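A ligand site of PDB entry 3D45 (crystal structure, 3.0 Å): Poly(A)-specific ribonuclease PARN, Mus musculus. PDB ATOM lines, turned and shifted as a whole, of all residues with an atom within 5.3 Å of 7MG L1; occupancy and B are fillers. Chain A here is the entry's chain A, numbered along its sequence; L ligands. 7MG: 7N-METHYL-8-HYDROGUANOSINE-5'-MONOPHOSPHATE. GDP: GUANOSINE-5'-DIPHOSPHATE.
Asn 335 touches 7MG L1.
Ser 337 touches 7MG L1 (OG to OP1, 3.9 Å).
CA of Lys 452 touches O6 of 7MG L1, at 3.4 Å.
Thr 453 touches 7MG L1 (N to O6, 3.6 Å).
CB of Trp 470 touches O4' of 7MG L1, 3.1 Å away.
Hydrophobic or aromatic side chains within 4 Å of 7MG L1: Trp 470.
Along chain A the residues within 4 Å of 7MG L1 span positions 321 to 473.
O2B of GDP L2 lies close to O5' of 7MG L1, 2.6 Å away.
The backbone carbonyl oxygen (O) of Asn 334 sits at hydrogen-bond distance from the side-chain hydroxyl (OG1) of Thr 453 (2.8 Å).
The side-chain carboxylate (OD1) of Asp 472 sits at hydrogen-bond distance from the side-chain hydroxyl (OG1) of Thr 474, 3.1 Å away.
The backbone NH (N) of Ser 337 sits close to the side-chain amide nitrogen (ND2) of Asn 335, at 3.2 Å.
The side-chain carboxylate of Glu 450 is in salt-bridge range of the side-chain amino group of Lys 449, at 3.0 Å.
NZ of Lys 321 lies within hydrogen-bond range of O of Thr 336 (3.2 Å).
OP2 of 7MG L1 is in salt-bridge range of NZ of Lys 321 (3.3 Å).
NH2 of Arg 421 lies within hydrogen-bond range of O6 of GDP L2.
The side-chain hydroxyl (OG) of Ser 337 is in hydrogen-bond range of an oxygen (O2B) of GDP L2 (3.4 Å).
The side-chain sulfur (SD) of Met 420 lies close to a nitrogen (N1) of GDP L2 (3.7 Å).
The side-chain carboxylate of Asp 473 sits at hydrogen-bond distance from an oxygen (O2') of 7MG L1.
O of Asp 472 lies close to O4' of 7MG L1 (2.7 Å).
The backbone carbonyl oxygen (O) of Lys 449 is in hydrogen-bond range of a nitrogen (N2) of 7MG L1, 3.2 Å away.
NZ of Lys 321 is in salt-bridge range of O2A of GDP L2.
The backbone carbonyl oxygen (O) of Asp 473 lies within hydrogen-bond range of a nitrogen (N2) of 7MG L1 (2.4 Å).
The backbone carbonyl oxygen (O) of Trp 451 is in hydrogen-bond range of a nitrogen (N1) of 7MG L1.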
ATOM      1  N   LYS A 321     -25.994   5.264   9.805  1.00  0.00           N
ATOM      2  CA  LYS A 321     -26.281   5.911  11.063  1.00  0.00           C
ATOM      3  C   LYS A 321     -26.997   7.257  10.858  1.00  0.00           C
ATOM      4  O   LYS A 321     -27.808   7.659  11.686  1.00  0.00           O
ATOM      5  CB  LYS A 321     -24.995   6.076  11.859  1.00  0.00           C
ATOM      6  CG  LYS A 321     -25.129   6.841  13.158  1.00  0.00           C
ATOM      7  CD  LYS A 321     -23.823   6.811  13.935  1.00  0.00           C
ATOM      8  CE  LYS A 321     -24.018   7.238  15.375  1.00  0.00           C
ATOM      9  NZ  LYS A 321     -24.512   6.137  16.243  1.00  0.00           N
ATOM     10  N   ASN A 334     -34.740   4.625  18.451  1.00  0.00           N
ATOM     11  CA  ASN A 334     -34.154   5.455  19.505  1.00  0.00           C
ATOM     12  C   ASN A 334     -32.672   5.222  19.875  1.00  0.00           C
ATOM     13  O   ASN A 334     -32.067   6.047  20.579  1.00  0.00           O
ATOM     14  CB  ASN A 334     -35.070   5.530  20.712  1.00  0.00           C
ATOM     15  CG  ASN A 334     -36.273   6.413  20.454  1.00  0.00           C
ATOM     16  OD1 ASN A 334     -36.132   7.540  19.950  1.00  0.00           O
ATOM     17  ND2 ASN A 334     -37.461   5.887  20.748  1.00  0.00           N
ATOM     18  N   ASN A 335     -32.098   4.141  19.378  1.00  0.00           N
ATOM     19  CA  ASN A 335     -30.667   3.947  19.490  1.00  0.00           C
ATOM     20  C   ASN A 335     -30.067   3.551  18.147  1.00  0.00           C
ATOM     21  O   ASN A 335     -30.554   2.615  17.505  1.00  0.00           O
ATOM     22  CB  ASN A 335     -30.318   2.925  20.547  1.00  0.00           C
ATOM     23  CG  ASN A 335     -28.839   2.693  20.621  1.00  0.00           C
ATOM     24  OD1 ASN A 335     -28.103   3.464  21.229  1.00  0.00           O
ATOM     25  ND2 ASN A 335     -28.369   1.654  19.944  1.00  0.00           N
ATOM     26  N   THR A 336     -29.014   4.260  17.742  1.00  0.00           N
ATOM     27  CA  THR A 336     -28.444   4.035  16.406  1.00  0.00           C
ATOM     28  C   THR A 336     -27.051   3.430  16.391  1.00  0.00           C
ATOM     29  O   THR A 336     -26.321   3.590  15.434  1.00  0.00           O
ATOM     30  CB  THR A 336     -28.504   5.294  15.508  1.00  0.00           C
ATOM     31  OG1 THR A 336     -27.735   6.343  16.080  1.00  0.00           O
ATOM     32  CG2 THR A 336     -29.898   5.779  15.367  1.00  0.00           C
ATOM     33  N   SER A 337     -26.675   2.748  17.475  1.00  0.00           N
ATOM     34  CA  SER A 337     -25.531   1.823  17.493  1.00  0.00           C
ATOM     35  C   SER A 337     -25.792   0.822  16.402  1.00  0.00           C
ATOM     36  O   SER A 337     -26.921   0.370  16.225  1.00  0.00           O
ATOM     37  CB  SER A 337     -25.461   0.996  18.791  1.00  0.00           C
ATOM     38  OG  SER A 337     -25.181   1.781  19.924  1.00  0.00           O
ATOM     39  N   MET A 420     -20.521  13.380  15.106  1.00  0.00           N
ATOM     40  CA  MET A 420     -20.660  13.062  16.533  1.00  0.00           C
ATOM     41  C   MET A 420     -20.582  14.291  17.470  1.00  0.00           C
ATOM     42  O   MET A 420     -19.933  15.320  17.155  1.00  0.00           O
ATOM     43  CB  MET A 420     -19.653  11.983  16.949  1.00  0.00           C
ATOM     44  CG  MET A 420     -20.264  10.630  17.144  1.00  0.00           C
ATOM     45  SD  MET A 420     -19.054   9.343  17.447  1.00  0.00           S
ATOM     46  CE  MET A 420     -20.094   8.083  18.172  1.00  0.00           C
ATOM     47  N   ARG A 421     -21.256  14.216  18.618  1.00  0.00           N
ATOM     48  CA  ARG A 421     -20.979  15.155  19.691  1.00  0.00           C
ATOM     49  C   ARG A 421     -20.904  16.583  19.207  1.00  0.00           C
ATOM     50  O   ARG A 421     -19.894  17.259  19.442  1.00  0.00           O
ATOM     51  CB  ARG A 421     -19.623  14.829  20.316  1.00  0.00           C
ATOM     52  CG  ARG A 421     -19.666  13.933  21.515  1.00  0.00           C
ATOM     53  CD  ARG A 421     -18.272  13.529  21.890  1.00  0.00           C
ATOM     54  NE  ARG A 421     -17.764  12.634  20.866  1.00  0.00           N
ATOM     55  CZ  ARG A 421     -18.075  11.345  20.798  1.00  0.00           C
ATOM     56  NH1 ARG A 421     -18.891  10.798  21.698  1.00  0.00           N
ATOM     57  NH2 ARG A 421     -17.577  10.611  19.822  1.00  0.00           N
ATOM     58  N   PHE A 447     -27.297  14.513  33.011  1.00  0.00           N
ATOM     59  CA  PHE A 447     -28.379  13.689  33.617  1.00  0.00           C
ATOM     60  C   PHE A 447     -27.896  12.329  34.121  1.00  0.00           C
ATOM     61  O   PHE A 447     -26.806  11.889  33.779  1.00  0.00           O
ATOM     62  CB  PHE A 447     -29.504  13.475  32.598  1.00  0.00           C
ATOM     63  CG  PHE A 447     -29.007  13.208  31.214  1.00  0.00           C
ATOM     64  CD1 PHE A 447     -28.803  14.248  30.314  1.00  0.00           C
ATOM     65  CD2 PHE A 447     -28.717  11.903  30.810  1.00  0.00           C
ATOM     66  CE1 PHE A 447     -28.328  13.994  29.033  1.00  0.00           C
ATOM     67  CE2 PHE A 447     -28.232  11.640  29.525  1.00  0.00           C
ATOM     68  CZ  PHE A 447     -28.039  12.691  28.643  1.00  0.00           C
ATOM     69  N   PRO A 448     -28.720  11.645  34.953  1.00  0.00           N
ATOM     70  CA  PRO A 448     -28.296  10.307  35.352  1.00  0.00           C
ATOM     71  C   PRO A 448     -27.995   9.463  34.132  1.00  0.00           C
ATOM     72  O   PRO A 448     -28.743   9.481  33.141  1.00  0.00           O
ATOM     73  CB  PRO A 448     -29.520   9.747  36.087  1.00  0.00           C
ATOM     74  CG  PRO A 448     -30.195  10.940  36.625  1.00  0.00           C
ATOM     75  CD  PRO A 448     -29.989  12.018  35.582  1.00  0.00           C
ATOM     76  N   LYS A 449     -26.887   8.748  34.215  1.00  0.00           N
ATOM     77  CA  LYS A 449     -26.510   7.778  33.197  1.00  0.00           C
ATOM     78  C   LYS A 449     -27.685   6.821  32.892  1.00  0.00           C
ATOM     79  O   LYS A 449     -27.676   6.168  31.848  1.00  0.00           O
ATOM     80  CB  LYS A 449     -25.284   6.961  33.637  1.00  0.00           C
ATOM     81  CG  LYS A 449     -24.464   7.522  34.792  1.00  0.00           C
ATOM     82  CD  LYS A 449     -24.980   7.004  36.128  1.00  0.00           C
ATOM     83  CE  LYS A 449     -24.423   7.766  37.303  1.00  0.00           C
ATOM     84  NZ  LYS A 449     -25.520   8.074  38.263  1.00  0.00           N
ATOM     85  N   GLU A 450     -28.686   6.750  33.768  1.00  0.00           N
ATOM     86  CA  GLU A 450     -29.721   5.749  33.591  1.00  0.00           C
ATOM     87  C   GLU A 450     -30.737   6.195  32.564  1.00  0.00           C
ATOM     88  O   GLU A 450     -31.646   5.439  32.239  1.00  0.00           O
ATOM     89  CB  GLU A 450     -30.406   5.351  34.914  1.00  0.00           C
ATOM     90  CG  GLU A 450     -29.797   5.859  36.234  1.00  0.00           C
ATOM     91  CD  GLU A 450     -28.317   5.524  36.431  1.00  0.00           C
ATOM     92  OE1 GLU A 450     -27.818   4.537  35.845  1.00  0.00           O
ATOM     93  OE2 GLU A 450     -27.649   6.264  37.178  1.00  0.00           O
ATOM     94  N   TRP A 451     -30.583   7.405  32.050  1.00  0.00           N
ATOM     95  CA  TRP A 451     -31.455   7.889  30.967  1.00  0.00           C
ATOM     96  C   TRP A 451     -31.232   7.158  29.654  1.00  0.00           C
ATOM     97  O   TRP A 451     -30.119   6.831  29.285  1.00  0.00           O
ATOM     98  CB  TRP A 451     -31.317   9.395  30.747  1.00  0.00           C
ATOM     99  CG  TRP A 451     -31.811  10.191  31.896  1.00  0.00           C
ATOM    100  CD1 TRP A 451     -31.868   9.794  33.194  1.00  0.00           C
ATOM    101  CD2 TRP A 451     -32.301  11.538  31.869  1.00  0.00           C
ATOM    102  NE1 TRP A 451     -32.370  10.793  33.973  1.00  0.00           N
ATOM    103  CE2 TRP A 451     -32.648  11.885  33.190  1.00  0.00           C
ATOM    104  CE3 TRP A 451     -32.493  12.484  30.860  1.00  0.00           C
ATOM    105  CZ2 TRP A 451     -33.166  13.135  33.526  1.00  0.00           C
ATOM    106  CZ3 TRP A 451     -33.012  13.734  31.196  1.00  0.00           C
ATOM    107  CH2 TRP A 451     -33.343  14.043  32.518  1.00  0.00           C
ATOM    108  N   LYS A 452     -32.333   6.891  28.957  1.00  0.00           N
ATOM    109  CA  LYS A 452     -32.310   6.365  27.614  1.00  0.00           C
ATOM    110  C   LYS A 452     -33.016   7.393  26.750  1.00  0.00           C
ATOM    111  O   LYS A 452     -33.732   8.235  27.276  1.00  0.00           O
ATOM    112  CB  LYS A 452     -32.996   4.987  27.563  1.00  0.00           C
ATOM    113  CG  LYS A 452     -32.204   3.947  28.326  1.00  0.00           C
ATOM    114  CD  LYS A 452     -32.611   2.526  28.076  1.00  0.00           C
ATOM    115  CE  LYS A 452     -31.785   1.622  28.990  1.00  0.00           C
ATOM    116  NZ  LYS A 452     -31.561   0.237  28.494  1.00  0.00           N
ATOM    117  N   THR A 453     -32.802   7.364  25.443  1.00  0.00           N
ATOM    118  CA  THR A 453     -33.259   8.449  24.578  1.00  0.00           C
ATOM    119  C   THR A 453     -34.708   8.910  24.836  1.00  0.00           C
ATOM    120  O   THR A 453     -34.984  10.119  24.910  1.00  0.00           O
ATOM    121  CB  THR A 453     -33.017   8.105  23.089  1.00  0.00           C
ATOM    122  OG1 THR A 453     -31.683   7.587  22.924  1.00  0.00           O
ATOM    123  CG2 THR A 453     -33.222   9.334  22.182  1.00  0.00           C
ATOM    124  N   TRP A 470     -25.973  12.918  21.445  1.00  0.00           N
ATOM    125  CA  TRP A 470     -25.211  12.388  22.563  1.00  0.00           C
ATOM    126  C   TRP A 470     -23.785  12.930  22.640  1.00  0.00           C
ATOM    127  O   TRP A 470     -23.039  12.836  21.686  1.00  0.00           O
ATOM    128  CB  TRP A 470     -25.196  10.861  22.490  1.00  0.00           C
ATOM    129  CG  TRP A 470     -26.564  10.290  22.664  1.00  0.00           C
ATOM    130  CD1 TRP A 470     -27.418   9.859  21.701  1.00  0.00           C
ATOM    131  CD2 TRP A 470     -27.239  10.096  23.901  1.00  0.00           C
ATOM    132  NE1 TRP A 470     -28.587   9.412  22.254  1.00  0.00           N
ATOM    133  CE2 TRP A 470     -28.501   9.548  23.611  1.00  0.00           C
ATOM    134  CE3 TRP A 470     -26.896  10.340  25.236  1.00  0.00           C
ATOM    135  CZ2 TRP A 470     -29.421   9.235  24.606  1.00  0.00           C
ATOM    136  CZ3 TRP A 470     -27.816  10.034  26.216  1.00  0.00           C
ATOM    137  CH2 TRP A 470     -29.061   9.485  25.899  1.00  0.00           C
ATOM    138  N   ILE A 471     -23.419  13.515  23.770  1.00  0.00           N
ATOM    139  CA  ILE A 471     -22.047  13.983  24.015  1.00  0.00           C
ATOM    140  C   ILE A 471     -21.353  12.926  24.846  1.00  0.00           C
ATOM    141  O   ILE A 471     -20.253  12.493  24.533  1.00  0.00           O
ATOM    142  CB  ILE A 471     -21.956  15.350  24.783  1.00  0.00           C
ATOM    143  CG1 ILE A 471     -22.865  16.414  24.166  1.00  0.00           C
ATOM    144  CG2 ILE A 471     -20.532  15.886  24.760  1.00  0.00           C
ATOM    145  CD1 ILE A 471     -23.197  17.516  25.121  1.00  0.00           C
ATOM    146  N   ASP A 472     -22.008  12.497  25.896  1.00  0.00           N
ATOM    147  CA  ASP A 472     -21.336  11.629  26.826  1.00  0.00           C
ATOM    148  C   ASP A 472     -22.077  10.320  26.937  1.00  0.00           C
ATOM    149  O   ASP A 472     -22.632   9.812  25.978  1.00  0.00           O
ATOM    150  CB  ASP A 472     -21.291  12.297  28.201  1.00  0.00           C
ATOM    151  CG  ASP A 472     -19.964  12.104  28.911  1.00  0.00           C
ATOM    152  OD1 ASP A 472     -19.947  12.177  30.158  1.00  0.00           O
ATOM    153  OD2 ASP A 472     -18.944  11.871  28.233  1.00  0.00           O
ATOM    154  N   ASP A 473     -22.051   9.812  28.155  1.00  0.00           N
ATOM    155  CA  ASP A 473     -22.874   8.725  28.569  1.00  0.00           C
ATOM    156  C   ASP A 473     -23.872   9.416  29.487  1.00  0.00           C
ATOM    157  O   ASP A 473     -24.960   8.898  29.780  1.00  0.00           O
ATOM    158  CB  ASP A 473     -21.986   7.747  29.343  1.00  0.00           C
ATOM    159  CG  ASP A 473     -22.483   6.308  29.271  1.00  0.00           C
ATOM    160  OD1 ASP A 473     -21.842   5.520  28.539  1.00  0.00           O
ATOM    161  OD2 ASP A 473     -23.502   5.983  29.943  1.00  0.00           O
ATOM    162  N   THR A 474     -23.491  10.610  29.946  1.00  0.00           N
ATOM    163  CA  THR A 474     -24.277  11.355  30.945  1.00  0.00           C
ATOM    164  C   THR A 474     -24.677  12.732  30.450  1.00  0.00           C
ATOM    165  O   THR A 474     -25.124  13.568  31.239  1.00  0.00           O
ATOM    166  CB  THR A 474     -23.516  11.536  32.291  1.00  0.00           C
ATOM    167  OG1 THR A 474     -22.352  12.364  32.101  1.00  0.00           O
ATOM    168  CG2 THR A 474     -23.126  10.192  32.874  1.00  0.00           C
HETATM  169  P   7MG L   1     -24.228   6.556  19.680  1.00  0.00           P
HETATM  170  OP1 7MG L   1     -25.270   5.664  20.265  1.00  0.00           O
HETATM  171  OP2 7MG L   1     -24.506   7.889  19.094  1.00  0.00           O
HETATM  172  O5' 7MG L   1     -23.117   6.840  20.767  1.00  0.00           O
HETATM  173  C5' 7MG L   1     -23.415   7.972  21.491  1.00  0.00           C
HETATM  174  C4' 7MG L   1     -22.692   8.006  22.810  1.00  0.00           C
HETATM  175  O4' 7MG L   1     -23.632   8.530  23.775  1.00  0.00           O
HETATM  176  C3' 7MG L   1     -22.122   6.713  23.368  1.00  0.00           C
HETATM  177  O3' 7MG L   1     -20.898   7.062  23.920  1.00  0.00           O
HETATM  178  C2' 7MG L   1     -23.031   6.336  24.518  1.00  0.00           C
HETATM  179  O2' 7MG L   1     -22.332   6.224  25.732  1.00  0.00           O
HETATM  180  C1' 7MG L   1     -23.954   7.522  24.690  1.00  0.00           C
HETATM  181  N9  7MG L   1     -25.317   7.087  24.571  1.00  0.00           N
HETATM  182  C8  7MG L   1     -25.979   6.616  23.461  1.00  0.00           C
HETATM  183  N7  7MG L   1     -27.206   6.270  23.767  1.00  0.00           N
HETATM  184  C5  7MG L   1     -27.315   6.535  25.127  1.00  0.00           C
HETATM  185  C6  7MG L   1     -28.398   6.351  25.972  1.00  0.00           C
HETATM  186  O6  7MG L   1     -29.523   5.912  25.686  1.00  0.00           O
HETATM  187  N1  7MG L   1     -28.099   6.746  27.279  1.00  0.00           N
HETATM  188  C2  7MG L   1     -26.902   7.247  27.725  1.00  0.00           C
HETATM  189  N2  7MG L   1     -26.843   7.567  29.044  1.00  0.00           N
HETATM  190  N3  7MG L   1     -25.861   7.407  26.907  1.00  0.00           N
HETATM  191  C4  7MG L   1     -26.160   7.028  25.634  1.00  0.00           C
HETATM  192  CM7 7MG L   1     -28.289   5.801  22.899  1.00  0.00           C
HETATM  193  PB  GDP L   2     -21.934   4.806  18.980  1.00  0.00           P
HETATM  194  O1B GDP L   2     -20.693   5.377  19.603  1.00  0.00           O
HETATM  195  O2B GDP L   2     -22.859   4.323  20.071  1.00  0.00           O
HETATM  196  O3B GDP L   2     -22.526   5.885  18.103  1.00  0.00           O
HETATM  197  O3A GDP L   2     -21.599   3.503  18.112  1.00  0.00           O
HETATM  198  PA  GDP L   2     -21.929   3.397  16.543  1.00  0.00           P
HETATM  199  O1A GDP L   2     -21.822   1.933  16.135  1.00  0.00           O
HETATM  200  O2A GDP L   2     -23.235   4.028  16.133  1.00  0.00           O
HETATM  201  O5' GDP L   2     -20.652   4.195  15.991  1.00  0.00           O
HETATM  202  C5' GDP L   2     -19.384   3.761  16.446  1.00  0.00           C
HETATM  203  C4' GDP L   2     -18.331   3.995  15.387  1.00  0.00           C
HETATM  204  O4' GDP L   2     -18.013   5.380  15.341  1.00  0.00           O
HETATM  205  C3' GDP L   2     -17.063   3.281  15.775  1.00  0.00           C
HETATM  206  O3' GDP L   2     -16.948   2.171  14.898  1.00  0.00           O
HETATM  207  C2' GDP L   2     -15.936   4.280  15.598  1.00  0.00           C
HETATM  208  O2' GDP L   2     -15.067   3.902  14.537  1.00  0.00           O
HETATM  209  C1' GDP L   2     -16.612   5.570  15.198  1.00  0.00           C
HETATM  210  N9  GDP L   2     -16.147   6.719  16.023  1.00  0.00           N
HETATM  211  C8  GDP L   2     -15.495   6.676  17.213  1.00  0.00           C
HETATM  212  N7  GDP L   2     -15.197   7.916  17.668  1.00  0.00           N
HETATM  213  C5  GDP L   2     -15.669   8.786  16.767  1.00  0.00           C
HETATM  214  C6  GDP L   2     -15.698  10.260  16.607  1.00  0.00           C
HETATM  215  O6  GDP L   2     -15.209  10.996  17.466  1.00  0.00           O
HETATM  216  N1  GDP L   2     -16.276  10.791  15.530  1.00  0.00           N
HETATM  217  C2  GDP L   2     -16.826  10.008  14.590  1.00  0.00           C
HETATM  218  N2  GDP L   2     -17.395  10.626  13.531  1.00  0.00           N
HETATM  219  N3  GDP L   2     -16.832   8.654  14.648  1.00  0.00           N
HETATM  220  C4  GDP L   2     -16.289   7.997  15.687  1.00  0.00           C
